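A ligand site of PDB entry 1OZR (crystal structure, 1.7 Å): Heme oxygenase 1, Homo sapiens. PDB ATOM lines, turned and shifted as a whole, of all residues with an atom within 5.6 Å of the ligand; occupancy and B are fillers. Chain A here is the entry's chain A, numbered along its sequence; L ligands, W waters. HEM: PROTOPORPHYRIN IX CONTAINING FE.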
ATOM      1  N   SER A  14      10.683  10.159 -21.277  1.00  0.00           N
ATOM      2  CA  SER A  14      10.078  10.877 -20.163  1.00  0.00           C
ATOM      3  C   SER A  14       8.555  10.782 -20.215  1.00  0.00           C
ATOM      4  O   SER A  14       7.895  10.625 -19.192  1.00  0.00           O
ATOM      5  CB  SER A  14      10.506  12.347 -20.167  1.00  0.00           C
ATOM      6  OG  SER A  14      10.076  13.001 -21.341  1.00  0.00           O
ATOM      7  N   LEU A  17       7.455   7.106 -19.492  1.00  0.00           N
ATOM      8  CA  LEU A  17       7.510   6.785 -18.066  1.00  0.00           C
ATOM      9  C   LEU A  17       6.309   7.341 -17.317  1.00  0.00           C
ATOM     10  O   LEU A  17       5.657   6.631 -16.556  1.00  0.00           O
ATOM     11  CB  LEU A  17       8.800   7.335 -17.456  1.00  0.00           C
ATOM     12  CG  LEU A  17      10.091   6.582 -17.796  1.00  0.00           C
ATOM     13  CD1 LEU A  17      11.292   7.407 -17.373  1.00  0.00           C
ATOM     14  CD2 LEU A  17      10.080   5.232 -17.095  1.00  0.00           C
ATOM     15  N   LYS A  18       6.013   8.620 -17.543  1.00  0.00           N
ATOM     16  CA  LYS A  18       4.883   9.260 -16.874  1.00  0.00           C
ATOM     17  C   LYS A  18       3.577   8.541 -17.192  1.00  0.00           C
ATOM     18  O   LYS A  18       2.732   8.355 -16.304  1.00  0.00           O
ATOM     19  CB  LYS A  18       4.779  10.727 -17.305  1.00  0.00           C
ATOM     20  CG  LYS A  18       3.634  11.473 -16.645  1.00  0.00           C
ATOM     21  CD  LYS A  18       3.656  12.959 -16.957  1.00  0.00           C
ATOM     22  CE  LYS A  18       2.510  13.672 -16.246  1.00  0.00           C
ATOM     23  NZ  LYS A  18       2.511  15.146 -16.510  1.00  0.00           N
ATOM     24  N   HIS A  25       1.279   5.190  -9.507  1.00  0.00           N
ATOM     25  CA  HIS A  25       1.413   6.430  -8.754  1.00  0.00           C
ATOM     26  C   HIS A  25       0.149   6.638  -7.938  1.00  0.00           C
ATOM     27  O   HIS A  25       0.198   7.019  -6.771  1.00  0.00           O
ATOM     28  CB  HIS A  25       1.630   7.631  -9.680  1.00  0.00           C
ATOM     29  CG  HIS A  25       1.893   8.917  -8.959  1.00  0.00           C
ATOM     30  ND1 HIS A  25       0.901   9.640  -8.339  1.00  0.00           N
ATOM     31  CD2 HIS A  25       3.045   9.594  -8.725  1.00  0.00           C
ATOM     32  CE1 HIS A  25       1.422  10.706  -7.765  1.00  0.00           C
ATOM     33  NE2 HIS A  25       2.722  10.708  -7.991  1.00  0.00           N
ATOM     34  N   ALA A  28       0.101   4.460  -5.032  1.00  0.00           N
ATOM     35  CA  ALA A  28       0.931   5.028  -3.965  1.00  0.00           C
ATOM     36  C   ALA A  28       0.140   6.079  -3.198  1.00  0.00           C
ATOM     37  O   ALA A  28       0.191   6.138  -1.966  1.00  0.00           O
ATOM     38  CB  ALA A  28       2.194   5.631  -4.548  1.00  0.00           C
ATOM     39  N   GLU A  29      -0.589   6.922  -3.925  1.00  0.00           N
ATOM     40  CA  GLU A  29      -1.400   7.968  -3.308  1.00  0.00           C
ATOM     41  C   GLU A  29      -2.498   7.359  -2.450  1.00  0.00           C
ATOM     42  O   GLU A  29      -2.855   7.913  -1.407  1.00  0.00           O
ATOM     43  CB  GLU A  29      -2.052   8.847  -4.382  1.00  0.00           C
ATOM     44  CG  GLU A  29      -1.102   9.683  -5.225  1.00  0.00           C
ATOM     45  CD  GLU A  29      -1.831  10.474  -6.296  1.00  0.00           C
ATOM     46  OE1 GLU A  29      -2.632  11.360  -5.941  1.00  0.00           O
ATOM     47  OE2 GLU A  29      -1.608  10.200  -7.496  1.00  0.00           O
ATOM     48  N   MET A  34      -0.168   6.968   3.166  1.00  0.00           N
ATOM     49  CA  MET A  34      -0.138   8.218   2.414  1.00  0.00           C
ATOM     50  C   MET A  34      -1.490   8.921   2.398  1.00  0.00           C
ATOM     51  O   MET A  34      -1.553  10.143   2.317  1.00  0.00           O
ATOM     52  CB  MET A  34       0.343   7.962   0.985  1.00  0.00           C
ATOM     53  CG  MET A  34       1.833   7.685   0.891  1.00  0.00           C
ATOM     54  SD  MET A  34       2.853   9.134   1.279  1.00  0.00           S
ATOM     55  CE  MET A  34       3.010   8.986   3.001  1.00  0.00           C
ATOM     56  N   GLN A  38      -1.841  12.774   3.516  1.00  0.00           N
ATOM     57  CA  GLN A  38      -2.491  13.823   2.723  1.00  0.00           C
ATOM     58  C   GLN A  38      -3.599  14.526   3.507  1.00  0.00           C
ATOM     59  O   GLN A  38      -3.833  15.720   3.319  1.00  0.00           O
ATOM     60  CB  GLN A  38      -3.081  13.220   1.447  1.00  0.00           C
ATOM     61  CG  GLN A  38      -2.045  12.875   0.392  1.00  0.00           C
ATOM     62  CD  GLN A  38      -2.612  11.974  -0.681  1.00  0.00           C
ATOM     63  OE1 GLN A  38      -2.744  10.757  -0.481  1.00  0.00           O
ATOM     64  NE2 GLN A  38      -2.965  12.559  -1.815  1.00  0.00           N
ATOM     65  N   TYR A 114      14.155  -2.470  -0.590  1.00  0.00           N
ATOM     66  CA  TYR A 114      14.317  -1.358  -1.522  1.00  0.00           C
ATOM     67  C   TYR A 114      15.818  -1.148  -1.763  1.00  0.00           C
ATOM     68  O   TYR A 114      16.279  -1.068  -2.917  1.00  0.00           O
ATOM     69  CB  TYR A 114      13.674  -0.106  -0.902  1.00  0.00           C
ATOM     70  CG  TYR A 114      13.307   1.012  -1.857  1.00  0.00           C
ATOM     71  CD1 TYR A 114      13.997   1.202  -3.056  1.00  0.00           C
ATOM     72  CD2 TYR A 114      12.314   1.934  -1.521  1.00  0.00           C
ATOM     73  CE1 TYR A 114      13.713   2.292  -3.886  1.00  0.00           C
ATOM     74  CE2 TYR A 114      12.021   3.022  -2.328  1.00  0.00           C
ATOM     75  CZ  TYR A 114      12.728   3.200  -3.503  1.00  0.00           C
ATOM     76  OH  TYR A 114      12.453   4.298  -4.285  1.00  0.00           O
ATOM     77  N   TYR A 134      14.789   8.678 -11.512  1.00  0.00           N
ATOM     78  CA  TYR A 134      13.581   9.351 -11.979  1.00  0.00           C
ATOM     79  C   TYR A 134      12.484   9.309 -10.921  1.00  0.00           C
ATOM     80  O   TYR A 134      11.973  10.352 -10.494  1.00  0.00           O
ATOM     81  CB  TYR A 134      13.061   8.661 -13.254  1.00  0.00           C
ATOM     82  CG  TYR A 134      11.602   8.934 -13.567  1.00  0.00           C
ATOM     83  CD1 TYR A 134      11.204  10.161 -14.094  1.00  0.00           C
ATOM     84  CD2 TYR A 134      10.628   7.966 -13.339  1.00  0.00           C
ATOM     85  CE1 TYR A 134       9.862  10.422 -14.382  1.00  0.00           C
ATOM     86  CE2 TYR A 134       9.272   8.214 -13.616  1.00  0.00           C
ATOM     87  CZ  TYR A 134       8.898   9.443 -14.138  1.00  0.00           C
ATOM     88  OH  TYR A 134       7.571   9.704 -14.397  1.00  0.00           O
ATOM     89  N   THR A 135      12.122   8.100 -10.514  1.00  0.00           N
ATOM     90  CA  THR A 135      11.077   7.871  -9.526  1.00  0.00           C
ATOM     91  C   THR A 135      11.281   8.654  -8.225  1.00  0.00           C
ATOM     92  O   THR A 135      10.362   9.301  -7.730  1.00  0.00           O
ATOM     93  CB  THR A 135      10.965   6.357  -9.218  1.00  0.00           C
ATOM     94  OG1 THR A 135      10.531   5.663 -10.395  1.00  0.00           O
ATOM     95  CG2 THR A 135       9.952   6.093  -8.086  1.00  0.00           C
ATOM     96  N   ARG A 136      12.500   8.613  -7.682  1.00  0.00           N
ATOM     97  CA  ARG A 136      12.812   9.320  -6.443  1.00  0.00           C
ATOM     98  C   ARG A 136      12.984  10.829  -6.572  1.00  0.00           C
ATOM     99  O   ARG A 136      12.231  11.600  -5.962  1.00  0.00           O
ATOM    100  CB  ARG A 136      14.076   8.720  -5.807  1.00  0.00           C
ATOM    101  CG  ARG A 136      13.826   7.532  -4.889  1.00  0.00           C
ATOM    102  CD  ARG A 136      13.745   7.945  -3.424  1.00  0.00           C
ATOM    103  NE  ARG A 136      12.546   8.713  -3.085  1.00  0.00           N
ATOM    104  CZ  ARG A 136      11.384   8.177  -2.726  1.00  0.00           C
ATOM    105  NH1 ARG A 136      11.259   6.858  -2.649  1.00  0.00           N
ATOM    106  NH2 ARG A 136      10.360   8.957  -2.385  1.00  0.00           N
ATOM    107  N   LEU A 138      12.500  13.102  -9.244  1.00  0.00           N
ATOM    108  CA  LEU A 138      11.400  13.850  -9.843  1.00  0.00           C
ATOM    109  C   LEU A 138      10.152  13.817  -8.974  1.00  0.00           C
ATOM    110  O   LEU A 138       9.394  14.788  -8.924  1.00  0.00           O
ATOM    111  CB  LEU A 138      11.077  13.332 -11.247  1.00  0.00           C
ATOM    112  CG  LEU A 138      11.720  14.146 -12.372  1.00  0.00           C
ATOM    113  CD1 LEU A 138      13.229  14.207 -12.159  1.00  0.00           C
ATOM    114  CD2 LEU A 138      11.383  13.514 -13.714  1.00  0.00           C
ATOM    115  N   GLY A 139       9.943  12.699  -8.292  1.00  0.00           N
ATOM    116  CA  GLY A 139       8.798  12.585  -7.425  1.00  0.00           C
ATOM    117  C   GLY A 139       8.905  13.489  -6.218  1.00  0.00           C
ATOM    118  O   GLY A 139       7.977  14.222  -5.894  1.00  0.00           O
ATOM    119  N   ASP A 140      10.051  13.436  -5.538  1.00  0.00           N
ATOM    120  CA  ASP A 140      10.258  14.267  -4.357  1.00  0.00           C
ATOM    121  C   ASP A 140      10.324  15.741  -4.726  1.00  0.00           C
ATOM    122  O   ASP A 140       9.936  16.603  -3.946  1.00  0.00           O
ATOM    123  CB  ASP A 140      11.542  13.827  -3.627  1.00  0.00           C
ATOM    124  CG  ASP A 140      11.452  12.406  -3.087  1.00  0.00           C
ATOM    125  OD1 ASP A 140      10.335  11.948  -2.784  1.00  0.00           O
ATOM    126  OD2 ASP A 140      12.497  11.735  -2.952  1.00  0.00           O
ATOM    127  N   SER A 142       8.597  17.245  -7.171  1.00  0.00           N
ATOM    128  CA  SER A 142       7.278  17.785  -7.471  1.00  0.00           C
ATOM    129  C   SER A 142       6.232  17.401  -6.426  1.00  0.00           C
ATOM    130  O   SER A 142       5.525  18.253  -5.902  1.00  0.00           O
ATOM    131  CB  SER A 142       6.829  17.367  -8.876  1.00  0.00           C
ATOM    132  OG  SER A 142       7.052  15.985  -9.103  1.00  0.00           O
ATOM    133  N   GLY A 143       6.142  16.115  -6.112  1.00  0.00           N
ATOM    134  CA  GLY A 143       5.173  15.671  -5.124  1.00  0.00           C
ATOM    135  C   GLY A 143       5.569  16.057  -3.716  1.00  0.00           C
ATOM    136  O   GLY A 143       4.747  16.513  -2.915  1.00  0.00           O
ATOM    137  N   VAL A 146       4.249  19.360  -1.992  1.00  0.00           N
ATOM    138  CA  VAL A 146       2.924  19.496  -1.396  1.00  0.00           C
ATOM    139  C   VAL A 146       2.933  18.819  -0.034  1.00  0.00           C
ATOM    140  O   VAL A 146       2.247  19.245   0.896  1.00  0.00           O
ATOM    141  CB  VAL A 146       1.820  18.851  -2.271  1.00  0.00           C
ATOM    142  CG1 VAL A 146       1.901  19.395  -3.689  1.00  0.00           C
ATOM    143  CG2 VAL A 146       1.954  17.342  -2.268  1.00  0.00           C
ATOM    144  N   LEU A 147       3.721  17.752   0.080  1.00  0.00           N
ATOM    145  CA  LEU A 147       3.821  17.006   1.330  1.00  0.00           C
ATOM    146  C   LEU A 147       4.537  17.808   2.409  1.00  0.00           C
ATOM    147  O   LEU A 147       4.247  17.648   3.593  1.00  0.00           O
ATOM    148  CB  LEU A 147       4.546  15.678   1.092  1.00  0.00           C
ATOM    149  CG  LEU A 147       3.805  14.694   0.186  1.00  0.00           C
ATOM    150  CD1 LEU A 147       4.629  13.421   0.032  1.00  0.00           C
ATOM    151  CD2 LEU A 147       2.436  14.375   0.769  1.00  0.00           C
ATOM    152  N   LYS A 179      13.120  20.381 -13.968  1.00  0.00           N
ATOM    153  CA  LYS A 179      12.424  19.177 -14.371  1.00  0.00           C
ATOM    154  C   LYS A 179      12.330  19.065 -15.893  1.00  0.00           C
ATOM    155  O   LYS A 179      12.286  17.963 -16.428  1.00  0.00           O
ATOM    156  CB  LYS A 179      11.027  19.117 -13.742  1.00  0.00           C
ATOM    157  CG  LYS A 179      11.050  18.599 -12.306  1.00  0.00           C
ATOM    158  CD  LYS A 179       9.662  18.321 -11.767  1.00  0.00           C
ATOM    159  CE  LYS A 179       8.866  19.592 -11.571  1.00  0.00           C
ATOM    160  NZ  LYS A 179       7.515  19.276 -11.032  1.00  0.00           N
ATOM    161  N   ARG A 183      14.089  15.956 -17.946  1.00  0.00           N
ATOM    162  CA  ARG A 183      13.335  15.165 -18.917  1.00  0.00           C
ATOM    163  C   ARG A 183      14.108  15.130 -20.237  1.00  0.00           C
ATOM    164  O   ARG A 183      14.267  14.076 -20.845  1.00  0.00           O
ATOM    165  CB  ARG A 183      11.946  15.766 -19.140  1.00  0.00           C
ATOM    166  CG  ARG A 183      11.066  15.763 -17.893  1.00  0.00           C
ATOM    167  CD  ARG A 183       9.608  16.017 -18.237  1.00  0.00           C
ATOM    168  NE  ARG A 183       8.739  15.979 -17.062  1.00  0.00           N
ATOM    169  CZ  ARG A 183       8.514  17.020 -16.266  1.00  0.00           C
ATOM    170  NH1 ARG A 183       9.079  18.197 -16.525  1.00  0.00           N
ATOM    171  NH2 ARG A 183       7.720  16.895 -15.221  1.00  0.00           N
ATOM    172  N   ALA A 206       9.942   0.407  -8.868  1.00  0.00           N
ATOM    173  CA  ALA A 206      10.326   1.413  -7.881  1.00  0.00           C
ATOM    174  C   ALA A 206       9.078   1.830  -7.099  1.00  0.00           C
ATOM    175  O   ALA A 206       9.119   1.916  -5.865  1.00  0.00           O
ATOM    176  CB  ALA A 206      10.937   2.619  -8.570  1.00  0.00           C
ATOM    177  N   PHE A 207       7.974   2.084  -7.797  1.00  0.00           N
ATOM    178  CA  PHE A 207       6.747   2.468  -7.110  1.00  0.00           C
ATOM    179  C   PHE A 207       6.270   1.362  -6.183  1.00  0.00           C
ATOM    180  O   PHE A 207       5.815   1.629  -5.070  1.00  0.00           O
ATOM    181  CB  PHE A 207       5.631   2.824  -8.099  1.00  0.00           C
ATOM    182  CG  PHE A 207       5.701   4.220  -8.640  1.00  0.00           C
ATOM    183  CD1 PHE A 207       6.472   4.518  -9.758  1.00  0.00           C
ATOM    184  CD2 PHE A 207       5.016   5.255  -8.020  1.00  0.00           C
ATOM    185  CE1 PHE A 207       6.549   5.809 -10.254  1.00  0.00           C
ATOM    186  CE2 PHE A 207       5.081   6.556  -8.502  1.00  0.00           C
ATOM    187  CZ  PHE A 207       5.854   6.840  -9.625  1.00  0.00           C
ATOM    188  N   ASN A 210       8.073   1.270  -2.940  1.00  0.00           N
ATOM    189  CA  ASN A 210       7.629   2.352  -2.054  1.00  0.00           C
ATOM    190  C   ASN A 210       6.297   1.965  -1.406  1.00  0.00           C
ATOM    191  O   ASN A 210       6.097   2.151  -0.203  1.00  0.00           O
ATOM    192  CB  ASN A 210       7.456   3.662  -2.838  1.00  0.00           C
ATOM    193  CG  ASN A 210       8.760   4.397  -3.046  1.00  0.00           C
ATOM    194  OD1 ASN A 210       9.225   5.136  -2.171  1.00  0.00           O
ATOM    195  ND2 ASN A 210       9.356   4.219  -4.223  1.00  0.00           N
ATOM    196  N   PHE A 214       5.275   1.630   2.543  1.00  0.00           N
ATOM    197  CA  PHE A 214       4.169   2.323   3.198  1.00  0.00           C
ATOM    198  C   PHE A 214       3.297   1.339   3.953  1.00  0.00           C
ATOM    199  O   PHE A 214       2.804   1.639   5.039  1.00  0.00           O
ATOM    200  CB  PHE A 214       3.291   3.061   2.190  1.00  0.00           C
ATOM    201  CG  PHE A 214       3.988   4.158   1.441  1.00  0.00           C
ATOM    202  CD1 PHE A 214       5.059   4.841   2.005  1.00  0.00           C
ATOM    203  CD2 PHE A 214       3.561   4.528   0.171  1.00  0.00           C
ATOM    204  CE1 PHE A 214       5.691   5.882   1.323  1.00  0.00           C
ATOM    205  CE2 PHE A 214       4.181   5.559  -0.530  1.00  0.00           C
ATOM    206  CZ  PHE A 214       5.250   6.236   0.049  1.00  0.00           C
HETATM  207  CHA HEM L   1       4.773  13.845  -9.933  1.00  0.00           C
HETATM  208  CHB HEM L   1       1.879  14.483  -6.081  1.00  0.00           C
HETATM  209  CHC HEM L   1       3.621  10.395  -4.104  1.00  0.00           C
HETATM  210  CHD HEM L   1       6.630   9.867  -7.893  1.00  0.00           C
HETATM  211  C1A HEM L   1       3.825  14.357  -9.043  1.00  0.00           C
HETATM  212  C2A HEM L   1       3.078  15.593  -9.262  1.00  0.00           C
HETATM  213  C3A HEM L   1       2.291  15.788  -8.180  1.00  0.00           C
HETATM  214  C4A HEM L   1       2.523  14.656  -7.295  1.00  0.00           C
HETATM  215  CMA HEM L   1       1.316  16.948  -7.986  1.00  0.00           C
HETATM  216  CAA HEM L   1       3.162  16.497 -10.492  1.00  0.00           C
HETATM  217  CBA HEM L   1       2.539  15.890 -11.751  1.00  0.00           C
HETATM  218  CGA HEM L   1       2.946  16.630 -13.013  1.00  0.00           C
HETATM  219  O1A HEM L   1       2.687  17.844 -13.118  1.00  0.00           O
HETATM  220  C1B HEM L   1       2.070  13.395  -5.231  1.00  0.00           C
HETATM  221  C2B HEM L   1       1.358  13.228  -3.978  1.00  0.00           C
HETATM  222  C3B HEM L   1       1.879  12.129  -3.392  1.00  0.00           C
HETATM  223  C4B HEM L   1       2.864  11.555  -4.328  1.00  0.00           C
HETATM  224  CMB HEM L   1       0.198  14.069  -3.455  1.00  0.00           C
HETATM  225  CAB HEM L   1       1.555  11.705  -2.111  1.00  0.00           C
HETATM  226  CBB HEM L   1       0.726  10.539  -1.876  1.00  0.00           C
HETATM  227  C1C HEM L   1       4.614   9.916  -4.960  1.00  0.00           C
HETATM  228  C2C HEM L   1       5.460   8.752  -4.683  1.00  0.00           C
HETATM  229  C3C HEM L   1       6.331   8.631  -5.721  1.00  0.00           C
HETATM  230  C4C HEM L   1       6.009   9.712  -6.655  1.00  0.00           C
HETATM  231  CMC HEM L   1       5.365   7.782  -3.510  1.00  0.00           C
HETATM  232  CAC HEM L   1       7.271   7.619  -5.925  1.00  0.00           C
HETATM  233  CBC HEM L   1       8.383   7.348  -5.056  1.00  0.00           C
HETATM  234  C1D HEM L   1       6.311  10.851  -8.806  1.00  0.00           C
HETATM  235  C2D HEM L   1       7.001  11.035 -10.076  1.00  0.00           C
HETATM  236  C3D HEM L   1       6.496  12.157 -10.632  1.00  0.00           C
HETATM  237  C4D HEM L   1       5.495  12.675  -9.719  1.00  0.00           C
HETATM  238  CMD HEM L   1       8.162  10.228 -10.636  1.00  0.00           C
HETATM  239  CAD HEM L   1       6.998  12.701 -11.965  1.00  0.00           C
HETATM  240  CBD HEM L   1       5.939  12.702 -13.059  1.00  0.00           C
HETATM  241  CGD HEM L   1       6.514  13.036 -14.429  1.00  0.00           C
HETATM  242  O1D HEM L   1       7.134  12.155 -15.043  1.00  0.00           O
HETATM  243  O2D HEM L   1       6.350  14.190 -14.873  1.00  0.00           O
HETATM  244  NA  HEM L   1       3.461  13.764  -7.838  1.00  0.00           N
HETATM  245  NB  HEM L   1       2.967  12.352  -5.455  1.00  0.00           N
HETATM  246  NC  HEM L   1       4.960  10.500  -6.191  1.00  0.00           N
HETATM  247  ND  HEM L   1       5.363  11.845  -8.597  1.00  0.00           N
HETATM  248 FE   HEM L   1       4.095  12.041  -7.068  1.00  0.00          FE
HETATM  249  O   HOH W   1       7.418  11.281  -3.769  1.00  0.00           O
HETATM  250  O   HOH W   2       1.389  12.533 -10.559  1.00  0.00           O
HETATM  251  O   HOH W   3       9.568  10.416  -5.134  1.00  0.00           O
HETATM  252  O   HOH W   4       8.187  12.724 -17.457  1.00  0.00           O
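NE2 of His 25 binds FE of the ligand. O1D of the ligand lies within hydrogen-bond range of OH of Tyr 134 (2.6 Å). NH2 of Arg 183 lies within salt-bridge range of O2D of the ligand (3.1 Å).
The guanidinium group (NH1) of Arg 183 sits close to the backbone carbonyl oxygen (O) of Lys 179, 3.2 Å away. The side-chain hydroxyl (OG) of Ser 142 is in hydrogen-bond range of the backbone carbonyl oxygen (O) of Leu 138, 2.6 Å away. OD1 of Asn 210 lies within hydrogen-bond range of NH1 of Arg 136, 2.7 Å away. ND2 of Asn 210 sits at hydrogen-bond distance from OH of Tyr 114 (3.1 Å). O of Glu 29 lies close to OE1 of Gln 38, at 3.0 Å. NH1 of Arg 136 is in hydrogen-bond range of OH of Tyr 114 (3.3 Å). The side-chain carboxylate (OD1) of Asp 140 lies within salt-bridge range of the guanidinium group (NH2) of Arg 136 (3.0 Å). The backbone carbonyl oxygen of Met 34 sits close to the side-chain amide oxygen of Gln 38 (3.1 Å).
Lys 18 touches the ligand (CB to O1D, 3.6 Å). Ala 28 touches the ligand. Glu 29 touches the ligand (CA to CBB, 3.6 Å). Met 34 touches the ligand. Gln 38 touches the ligand (OE1 to CBB, 3.7 Å). Thr 135 touches the ligand (CG2 to CBC, 3.6 Å). Arg 136 touches the ligand. Gly 139 touches the ligand (CA to C1D, 3.3 Å). Ser 142 touches the ligand (OG to CHA, 3.2 Å). Gly 143 touches the ligand (CA to C4A, 3.6 Å). CG2 of Val 146 touches CMB of the ligand, at 3.9 Å. Phe 207 touches the ligand. ND2 of Asn 210 touches CBC of the ligand (3.4 Å). Phe 214 touches the ligand (CZ to CMC, 3.9 Å). Hydrophobic or aromatic side chains within 4 Å of the ligand: His 25, Ala 28, Met 34, Tyr 134, Val 146, Phe 207 and Phe 214.
Water W4 lies within hydrogen-bond range of an oxygen (O1D) of the ligand (2.7 Å), the backbone carbonyl oxygen of Ser 14 (2.7 Å) and the guanidinium group of Arg 183 (3.3 Å).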
